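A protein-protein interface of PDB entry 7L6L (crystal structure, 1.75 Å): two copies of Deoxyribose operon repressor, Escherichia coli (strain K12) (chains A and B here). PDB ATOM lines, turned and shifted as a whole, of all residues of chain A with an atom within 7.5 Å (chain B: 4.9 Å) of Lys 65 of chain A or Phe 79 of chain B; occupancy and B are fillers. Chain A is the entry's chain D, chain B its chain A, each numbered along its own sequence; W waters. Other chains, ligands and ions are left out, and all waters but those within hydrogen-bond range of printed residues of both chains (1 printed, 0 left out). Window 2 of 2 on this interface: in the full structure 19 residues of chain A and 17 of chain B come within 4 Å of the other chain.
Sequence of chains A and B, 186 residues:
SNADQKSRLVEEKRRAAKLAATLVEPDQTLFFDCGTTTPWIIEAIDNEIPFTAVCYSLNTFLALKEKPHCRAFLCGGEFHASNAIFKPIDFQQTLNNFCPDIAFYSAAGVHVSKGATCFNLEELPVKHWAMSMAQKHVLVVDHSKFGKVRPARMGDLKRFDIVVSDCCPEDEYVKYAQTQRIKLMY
N of Gly 77 of chain B is in hydrogen-bond range of O of Leu 74 of chain A (2.9 Å). The side-chain carboxylate of Glu 78 of chain B lies within salt-bridge range of the guanidinium group of Arg 71 of chain A, at 2.8 Å. N of Phe 79 of chain B lies within hydrogen-bond range of O of Ala 72 of chain A, 2.9 Å away.
The backbone carbonyl oxygen of Ala 84 of chain B lies within hydrogen-bond range of the backbone NH of Leu 58 of chain B, 2.8 Å away.
Among the printed residues, merely in contact across the chains: Phe 61 of chain A with Phe 79 of chain B (3.4 Å), Phe 61 of chain A with Phe 86 of chain B (3.7 Å), Lys 65 of chain A with Leu 58 of chain B (3.9 Å), Lys 65 of chain A with Phe 79 of chain B (3.7 Å), Ala 72 of chain A with Glu 78 of chain B (3.7 Å), Phe 73 of chain A with Gly 77 of chain B (3.3 Å), Phe 73 of chain A with Glu 78 of chain B (3.4 Å) and Leu 74 of chain A with Phe 86 of chain B (3.6 Å).
Of chain B, only Leu 58 and Phe 79 come within 4 Å of Lys 65 of chain A. Phe 79 of chain B touches three residues of chain A. Of the printed residues of chain B, Phe 73 of chain A touches Gly 77 (3.3 Å) and Glu 78 (3.4 Å). Of the printed residues of chain A, Glu 78 of chain B touches Arg 71 (2.8 Å), Ala 72 (3.7 Å) and Phe 73 (3.4 Å). Of the printed residues of chain B, Arg 71 of chain A touches Glu 78 (2.8 Å). Of the printed residues of chain B, Leu 74 of chain A touches Gly 77 and Phe 86. Of the printed residues of chain A, Phe 86 of chain B touches Phe 61 and Leu 74. The nearest printed residue of chain B that does not touch Lys 65 of chain A is Ala 84 of chain B (5.5 Å).
Of the 17 printed residues of chain A, 6 touch a printed residue of chain B. Hydrophobic or aromatic side chains of chain A within 4 Å of the printed part of chain B: Phe 61, Phe 73 and Leu 74. Printed residues of chain B that touch a printed residue of chain A: Leu 58, Gly 77, Glu 78, Phe 79 and Phe 86. Hydrophobic or aromatic side chains of chain B within 4 Å of the printed part of chain A: Leu 58, Phe 79 and Phe 86. Along chain B the printed residues that touch a printed residue of chain A span positions 58 to 86. Among the printed residues, Asp or Glu carboxylates within 4 Å of a Lys or Arg side-chain nitrogen of the other chain: Arg 71 of chain A with Glu 78 of chain B (2.8 Å).
No position is printed for both chains.
Water W1 lies within hydrogen-bond range of the backbone NH of Ala 72 of chain A and the backbone carbonyl oxygen of Phe 79 of chain B.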
ATOM      1  N   ILE A  42      13.419  -1.218 -26.034  1.00  0.00           N
ATOM      2  CA  ILE A  42      11.973  -0.865 -25.965  1.00  0.00           C
ATOM      3  C   ILE A  42      11.799   0.634 -26.229  1.00  0.00           C
ATOM      4  O   ILE A  42      10.890   0.993 -27.006  1.00  0.00           O
ATOM      5  CB  ILE A  42      11.401  -1.297 -24.606  1.00  0.00           C
ATOM      6  CG1 ILE A  42      11.478  -2.818 -24.455  1.00  0.00           C
ATOM      7  CG2 ILE A  42       9.983  -0.779 -24.427  1.00  0.00           C
ATOM      8  CD1 ILE A  42      11.308  -3.303 -23.030  1.00  0.00           C
ATOM      9  N   ASN A  59      11.707  -3.516 -14.365  1.00  0.00           N
ATOM     10  CA  ASN A  59      12.118  -2.336 -15.173  1.00  0.00           C
ATOM     11  C   ASN A  59      11.749  -2.571 -16.644  1.00  0.00           C
ATOM     12  O   ASN A  59      11.353  -1.597 -17.308  1.00  0.00           O
ATOM     13  CB  ASN A  59      13.596  -1.991 -14.998  1.00  0.00           C
ATOM     14  CG  ASN A  59      14.512  -3.126 -15.389  1.00  0.00           C
ATOM     15  OD1 ASN A  59      14.147  -4.297 -15.260  1.00  0.00           O
ATOM     16  ND2 ASN A  59      15.708  -2.788 -15.850  1.00  0.00           N
ATOM     17  N   THR A  60      11.875  -3.811 -17.127  1.00  0.00           N
ATOM     18  CA  THR A  60      11.509  -4.135 -18.533  1.00  0.00           C
ATOM     19  C   THR A  60      10.009  -3.885 -18.704  1.00  0.00           C
ATOM     20  O   THR A  60       9.610  -3.256 -19.690  1.00  0.00           O
ATOM     21  CB  THR A  60      11.849  -5.593 -18.865  1.00  0.00           C
ATOM     22  OG1 THR A  60      13.219  -5.800 -18.523  1.00  0.00           O
ATOM     23  CG2 THR A  60      11.613  -5.942 -20.317  1.00  0.00           C
ATOM     24  N   PHE A  61       9.216  -4.383 -17.761  1.00  0.00           N
ATOM     25  CA  PHE A  61       7.754  -4.187 -17.847  1.00  0.00           C
ATOM     26  C   PHE A  61       7.408  -2.692 -17.838  1.00  0.00           C
ATOM     27  O   PHE A  61       6.584  -2.267 -18.666  1.00  0.00           O
ATOM     28  CB  PHE A  61       7.015  -4.900 -16.714  1.00  0.00           C
ATOM     29  CG  PHE A  61       5.575  -4.479 -16.685  1.00  0.00           C
ATOM     30  CD1 PHE A  61       4.702  -4.909 -17.671  1.00  0.00           C
ATOM     31  CD2 PHE A  61       5.122  -3.578 -15.743  1.00  0.00           C
ATOM     32  CE1 PHE A  61       3.391  -4.459 -17.697  1.00  0.00           C
ATOM     33  CE2 PHE A  61       3.809  -3.141 -15.763  1.00  0.00           C
ATOM     34  CZ  PHE A  61       2.947  -3.585 -16.737  1.00  0.00           C
ATOM     35  N   LEU A  62       8.014  -1.918 -16.930  1.00  0.00           N
ATOM     36  CA  LEU A  62       7.674  -0.472 -16.830  1.00  0.00           C
ATOM     37  C   LEU A  62       7.991   0.230 -18.155  1.00  0.00           C
ATOM     38  O   LEU A  62       7.221   1.124 -18.508  1.00  0.00           O
ATOM     39  CB  LEU A  62       8.398   0.167 -15.643  1.00  0.00           C
ATOM     40  CG  LEU A  62       7.874  -0.251 -14.267  1.00  0.00           C
ATOM     41  CD1 LEU A  62       8.754   0.294 -13.160  1.00  0.00           C
ATOM     42  CD2 LEU A  62       6.429   0.194 -14.070  1.00  0.00           C
ATOM     43  N   ALA A  63       9.039  -0.204 -18.866  1.00  0.00           N
ATOM     44  CA  ALA A  63       9.369   0.404 -20.177  1.00  0.00           C
ATOM     45  C   ALA A  63       8.281   0.032 -21.195  1.00  0.00           C
ATOM     46  O   ALA A  63       7.904   0.904 -21.985  1.00  0.00           O
ATOM     47  CB  ALA A  63      10.738  -0.026 -20.642  1.00  0.00           C
ATOM     48  N   LEU A  64       7.797  -1.216 -21.178  1.00  0.00           N
ATOM     49  CA  LEU A  64       6.721  -1.637 -22.119  1.00  0.00           C
ATOM     50  C   LEU A  64       5.443  -0.847 -21.824  1.00  0.00           C
ATOM     51  O   LEU A  64       4.754  -0.458 -22.777  1.00  0.00           O
ATOM     52  CB  LEU A  64       6.456  -3.141 -21.975  1.00  0.00           C
ATOM     53  CG  LEU A  64       7.575  -4.080 -22.421  1.00  0.00           C
ATOM     54  CD1 LEU A  64       7.199  -5.520 -22.101  1.00  0.00           C
ATOM     55  CD2 LEU A  64       7.874  -3.929 -23.902  1.00  0.00           C
ATOM     56  N   LYS A  65       5.157  -0.607 -20.542  1.00  0.00           N
ATOM     57  CA  LYS A  65       3.932   0.124 -20.123  1.00  0.00           C
ATOM     58  C   LYS A  65       3.897   1.529 -20.746  1.00  0.00           C
ATOM     59  O   LYS A  65       2.793   2.018 -20.997  1.00  0.00           O
ATOM     60  CB  LYS A  65       3.878   0.157 -18.592  1.00  0.00           C
ATOM     61  CG  LYS A  65       2.660   0.835 -17.977  1.00  0.00           C
ATOM     62  CD  LYS A  65       2.595   0.600 -16.479  1.00  0.00           C
ATOM     63  CE  LYS A  65       1.530   1.407 -15.772  1.00  0.00           C
ATOM     64  NZ  LYS A  65       1.893   2.839 -15.699  1.00  0.00           N
ATOM     65  N   GLU A  66       5.059   2.134 -21.012  1.00  0.00           N
ATOM     66  CA  GLU A  66       5.148   3.508 -21.581  1.00  0.00           C
ATOM     67  C   GLU A  66       4.943   3.495 -23.102  1.00  0.00           C
ATOM     68  O   GLU A  66       4.863   4.599 -23.682  1.00  0.00           O
ATOM     69  CB  GLU A  66       6.490   4.151 -21.220  1.00  0.00           C
ATOM     70  CG  GLU A  66       6.658   4.351 -19.727  1.00  0.00           C
ATOM     71  CD  GLU A  66       5.555   5.198 -19.122  1.00  0.00           C
ATOM     72  OE1 GLU A  66       5.259   6.260 -19.703  1.00  0.00           O
ATOM     73  OE2 GLU A  66       4.951   4.764 -18.119  1.00  0.00           O
ATOM     74  N   LYS A  67       4.875   2.317 -23.728  1.00  0.00           N
ATOM     75  CA  LYS A  67       4.676   2.239 -25.204  1.00  0.00           C
ATOM     76  C   LYS A  67       3.176   2.161 -25.477  1.00  0.00           C
ATOM     77  O   LYS A  67       2.549   1.134 -25.217  1.00  0.00           O
ATOM     78  CB  LYS A  67       5.400   1.029 -25.804  1.00  0.00           C
ATOM     79  CG  LYS A  67       6.876   0.903 -25.452  1.00  0.00           C
ATOM     80  CD  LYS A  67       7.755   2.012 -25.971  1.00  0.00           C
ATOM     81  CE  LYS A  67       7.880   2.015 -27.478  1.00  0.00           C
ATOM     82  NZ  LYS A  67       8.891   3.000 -27.924  1.00  0.00           N
ATOM     83  N   PRO A  68       2.562   3.236 -26.019  1.00  0.00           N
ATOM     84  CA  PRO A  68       1.123   3.269 -26.273  1.00  0.00           C
ATOM     85  C   PRO A  68       0.550   2.122 -27.115  1.00  0.00           C
ATOM     86  O   PRO A  68      -0.606   1.798 -26.912  1.00  0.00           O
ATOM     87  CB  PRO A  68       0.910   4.551 -27.095  1.00  0.00           C
ATOM     88  CG  PRO A  68       2.100   5.425 -26.772  1.00  0.00           C
ATOM     89  CD  PRO A  68       3.231   4.485 -26.420  1.00  0.00           C
ATOM     90  N   HIS A  69       1.347   1.548 -28.023  1.00  0.00           N
ATOM     91  CA  HIS A  69       0.813   0.497 -28.930  1.00  0.00           C
ATOM     92  C   HIS A  69       1.395  -0.878 -28.590  1.00  0.00           C
ATOM     93  O   HIS A  69       1.358  -1.770 -29.459  1.00  0.00           O
ATOM     94  CB  HIS A  69       1.024   0.910 -30.385  1.00  0.00           C
ATOM     95  CG  HIS A  69       0.317   2.183 -30.703  1.00  0.00           C
ATOM     96  ND1 HIS A  69      -1.061   2.273 -30.692  1.00  0.00           N
ATOM     97  CD2 HIS A  69       0.779   3.409 -31.027  1.00  0.00           C
ATOM     98  CE1 HIS A  69      -1.419   3.505 -30.997  1.00  0.00           C
ATOM     99  NE2 HIS A  69      -0.310   4.220 -31.210  1.00  0.00           N
ATOM    100  N   CYS A  70       1.876  -1.044 -27.362  1.00  0.00           N
ATOM    101  CA  CYS A  70       2.415  -2.358 -26.939  1.00  0.00           C
ATOM    102  C   CYS A  70       1.395  -3.105 -26.082  1.00  0.00           C
ATOM    103  O   CYS A  70       0.910  -2.524 -25.093  1.00  0.00           O
ATOM    104  CB  CYS A  70       3.692  -2.212 -26.125  1.00  0.00           C
ATOM    105  SG  CYS A  70       4.239  -3.766 -25.369  1.00  0.00           S
ATOM    106  N   ARG A  71       1.061  -4.328 -26.489  1.00  0.00           N
ATOM    107  CA  ARG A  71       0.236  -5.242 -25.662  1.00  0.00           C
ATOM    108  C   ARG A  71       1.257  -5.979 -24.786  1.00  0.00           C
ATOM    109  O   ARG A  71       2.005  -6.812 -25.339  1.00  0.00           O
ATOM    110  CB  ARG A  71      -0.586  -6.157 -26.567  1.00  0.00           C
ATOM    111  CG  ARG A  71      -1.522  -7.086 -25.819  1.00  0.00           C
ATOM    112  CD  ARG A  71      -2.223  -7.984 -26.810  1.00  0.00           C
ATOM    113  NE  ARG A  71      -3.199  -8.835 -26.156  1.00  0.00           N
ATOM    114  CZ  ARG A  71      -3.837  -9.835 -26.750  1.00  0.00           C
ATOM    115  NH1 ARG A  71      -3.583 -10.120 -28.018  1.00  0.00           N
ATOM    116  NH2 ARG A  71      -4.715 -10.552 -26.071  1.00  0.00           N
ATOM    117  N   ALA A  72       1.292  -5.667 -23.484  1.00  0.00           N
ATOM    118  CA  ALA A  72       2.357  -6.164 -22.584  1.00  0.00           C
ATOM    119  C   ALA A  72       1.898  -7.328 -21.696  1.00  0.00           C
ATOM    120  O   ALA A  72       0.795  -7.277 -21.123  1.00  0.00           O
ATOM    121  CB  ALA A  72       2.867  -5.017 -21.738  1.00  0.00           C
ATOM    122  N   PHE A  73       2.747  -8.349 -21.632  1.00  0.00           N
ATOM    123  CA  PHE A  73       2.558  -9.538 -20.771  1.00  0.00           C
ATOM    124  C   PHE A  73       3.738  -9.630 -19.813  1.00  0.00           C
ATOM    125  O   PHE A  73       4.888  -9.423 -20.245  1.00  0.00           O
ATOM    126  CB  PHE A  73       2.478 -10.819 -21.599  1.00  0.00           C
ATOM    127  CG  PHE A  73       1.216 -10.943 -22.404  1.00  0.00           C
ATOM    128  CD1 PHE A  73       1.070 -10.257 -23.596  1.00  0.00           C
ATOM    129  CD2 PHE A  73       0.179 -11.745 -21.967  1.00  0.00           C
ATOM    130  CE1 PHE A  73      -0.097 -10.364 -24.334  1.00  0.00           C
ATOM    131  CE2 PHE A  73      -0.988 -11.845 -22.701  1.00  0.00           C
ATOM    132  CZ  PHE A  73      -1.125 -11.157 -23.882  1.00  0.00           C
ATOM    133  N   LEU A  74       3.452  -9.936 -18.550  1.00  0.00           N
ATOM    134  CA  LEU A  74       4.523 -10.119 -17.542  1.00  0.00           C
ATOM    135  C   LEU A  74       4.477 -11.567 -17.051  1.00  0.00           C
ATOM    136  O   LEU A  74       3.368 -12.037 -16.712  1.00  0.00           O
ATOM    137  CB  LEU A  74       4.318  -9.139 -16.380  1.00  0.00           C
ATOM    138  CG  LEU A  74       5.289  -9.265 -15.201  1.00  0.00           C
ATOM    139  CD1 LEU A  74       6.739  -9.124 -15.642  1.00  0.00           C
ATOM    140  CD2 LEU A  74       4.970  -8.216 -14.144  1.00  0.00           C
ATOM    141  N   LEU B  58       0.044  -4.064 -10.210  1.00  0.00           N
ATOM    142  CA  LEU B  58       1.312  -3.302 -10.107  1.00  0.00           C
ATOM    143  C   LEU B  58       1.395  -2.482  -8.810  1.00  0.00           C
ATOM    144  O   LEU B  58       2.416  -2.609  -8.126  1.00  0.00           O
ATOM    145  CB  LEU B  58       1.423  -2.403 -11.342  1.00  0.00           C
ATOM    146  CG  LEU B  58       2.702  -1.579 -11.448  1.00  0.00           C
ATOM    147  CD1 LEU B  58       3.932  -2.474 -11.490  1.00  0.00           C
ATOM    148  CD2 LEU B  58       2.656  -0.682 -12.677  1.00  0.00           C
ATOM    149  N   GLY B  77       0.505 -12.321 -16.447  1.00  0.00           N
ATOM    150  CA  GLY B  77      -0.546 -12.384 -17.473  1.00  0.00           C
ATOM    151  C   GLY B  77      -0.538 -11.116 -18.300  1.00  0.00           C
ATOM    152  O   GLY B  77       0.499 -10.434 -18.305  1.00  0.00           O
ATOM    153  N   GLU B  78      -1.650 -10.826 -18.970  1.00  0.00           N
ATOM    154  CA  GLU B  78      -1.750  -9.607 -19.806  1.00  0.00           C
ATOM    155  C   GLU B  78      -2.019  -8.408 -18.894  1.00  0.00           C
ATOM    156  O   GLU B  78      -2.909  -8.506 -18.039  1.00  0.00           O
ATOM    157  CB  GLU B  78      -2.879  -9.766 -20.824  1.00  0.00           C
ATOM    158  CG  GLU B  78      -2.979  -8.600 -21.778  1.00  0.00           C
ATOM    159  CD  GLU B  78      -3.985  -8.784 -22.899  1.00  0.00           C
ATOM    160  OE1 GLU B  78      -4.582  -9.877 -22.990  1.00  0.00           O
ATOM    161  OE2 GLU B  78      -4.145  -7.842 -23.691  1.00  0.00           O
ATOM    162  N   PHE B  79      -1.294  -7.311 -19.103  1.00  0.00           N
ATOM    163  CA  PHE B  79      -1.502  -6.096 -18.279  1.00  0.00           C
ATOM    164  C   PHE B  79      -2.740  -5.337 -18.771  1.00  0.00           C
ATOM    165  O   PHE B  79      -2.898  -5.170 -19.997  1.00  0.00           O
ATOM    166  CB  PHE B  79      -0.272  -5.189 -18.333  1.00  0.00           C
ATOM    167  CG  PHE B  79      -0.407  -3.912 -17.544  1.00  0.00           C
ATOM    168  CD1 PHE B  79      -0.348  -3.927 -16.161  1.00  0.00           C
ATOM    169  CD2 PHE B  79      -0.571  -2.693 -18.185  1.00  0.00           C
ATOM    170  CE1 PHE B  79      -0.467  -2.755 -15.429  1.00  0.00           C
ATOM    171  CE2 PHE B  79      -0.685  -1.521 -17.452  1.00  0.00           C
ATOM    172  CZ  PHE B  79      -0.646  -1.557 -16.077  1.00  0.00           C
ATOM    173  N   HIS B  80      -3.591  -4.927 -17.829  1.00  0.00           N
ATOM    174  CA  HIS B  80      -4.801  -4.102 -18.100  1.00  0.00           C
ATOM    175  C   HIS B  80      -4.638  -2.807 -17.309  1.00  0.00           C
ATOM    176  O   HIS B  80      -4.460  -2.890 -16.079  1.00  0.00           O
ATOM    177  CB  HIS B  80      -6.089  -4.861 -17.760  1.00  0.00           C
ATOM    178  CG  HIS B  80      -6.343  -6.001 -18.682  1.00  0.00           C
ATOM    179  ND1 HIS B  80      -7.094  -5.862 -19.837  1.00  0.00           N
ATOM    180  CD2 HIS B  80      -5.923  -7.282 -18.652  1.00  0.00           C
ATOM    181  CE1 HIS B  80      -7.137  -7.023 -20.467  1.00  0.00           C
ATOM    182  NE2 HIS B  80      -6.428  -7.906 -19.763  1.00  0.00           N
ATOM    183  N   ALA B  81      -4.676  -1.669 -18.000  1.00  0.00           N
ATOM    184  CA  ALA B  81      -4.456  -0.350 -17.360  1.00  0.00           C
ATOM    185  C   ALA B  81      -5.388  -0.141 -16.164  1.00  0.00           C
ATOM    186  O   ALA B  81      -4.897   0.358 -15.136  1.00  0.00           O
ATOM    187  CB  ALA B  81      -4.624   0.756 -18.376  1.00  0.00           C
ATOM    188  N   ALA B  84      -4.422  -1.450 -12.962  1.00  0.00           N
ATOM    189  CA  ALA B  84      -3.052  -1.941 -13.252  1.00  0.00           C
ATOM    190  C   ALA B  84      -2.935  -3.431 -12.911  1.00  0.00           C
ATOM    191  O   ALA B  84      -1.975  -3.807 -12.203  1.00  0.00           O
ATOM    192  CB  ALA B  84      -2.054  -1.113 -12.468  1.00  0.00           C
ATOM    193  N   ILE B  85      -3.862  -4.246 -13.421  1.00  0.00           N
ATOM    194  CA  ILE B  85      -3.846  -5.701 -13.095  1.00  0.00           C
ATOM    195  C   ILE B  85      -3.181  -6.516 -14.203  1.00  0.00           C
ATOM    196  O   ILE B  85      -3.006  -6.017 -15.334  1.00  0.00           O
ATOM    197  CB  ILE B  85      -5.271  -6.251 -12.872  1.00  0.00           C
ATOM    198  CG1 ILE B  85      -6.076  -6.278 -14.176  1.00  0.00           C
ATOM    199  CG2 ILE B  85      -5.992  -5.491 -11.771  1.00  0.00           C
ATOM    200  CD1 ILE B  85      -7.211  -7.266 -14.160  1.00  0.00           C
ATOM    201  N   PHE B  86      -2.877  -7.760 -13.849  1.00  0.00           N
ATOM    202  CA  PHE B  86      -2.356  -8.792 -14.769  1.00  0.00           C
ATOM    203  C   PHE B  86      -3.428  -9.877 -14.817  1.00  0.00           C
ATOM    204  O   PHE B  86      -3.825 -10.375 -13.744  1.00  0.00           O
ATOM    205  CB  PHE B  86      -0.988  -9.305 -14.316  1.00  0.00           C
ATOM    206  CG  PHE B  86       0.066  -8.230 -14.311  1.00  0.00           C
ATOM    207  CD1 PHE B  86       0.738  -7.895 -15.477  1.00  0.00           C
ATOM    208  CD2 PHE B  86       0.349  -7.518 -13.159  1.00  0.00           C
ATOM    209  CE1 PHE B  86       1.695  -6.891 -15.480  1.00  0.00           C
ATOM    210  CE2 PHE B  86       1.299  -6.507 -13.167  1.00  0.00           C
ATOM    211  CZ  PHE B  86       1.977  -6.203 -14.325  1.00  0.00           C
HETATM  212  O   HOH W   1      -0.864  -4.299 -21.988  1.00  0.00           O
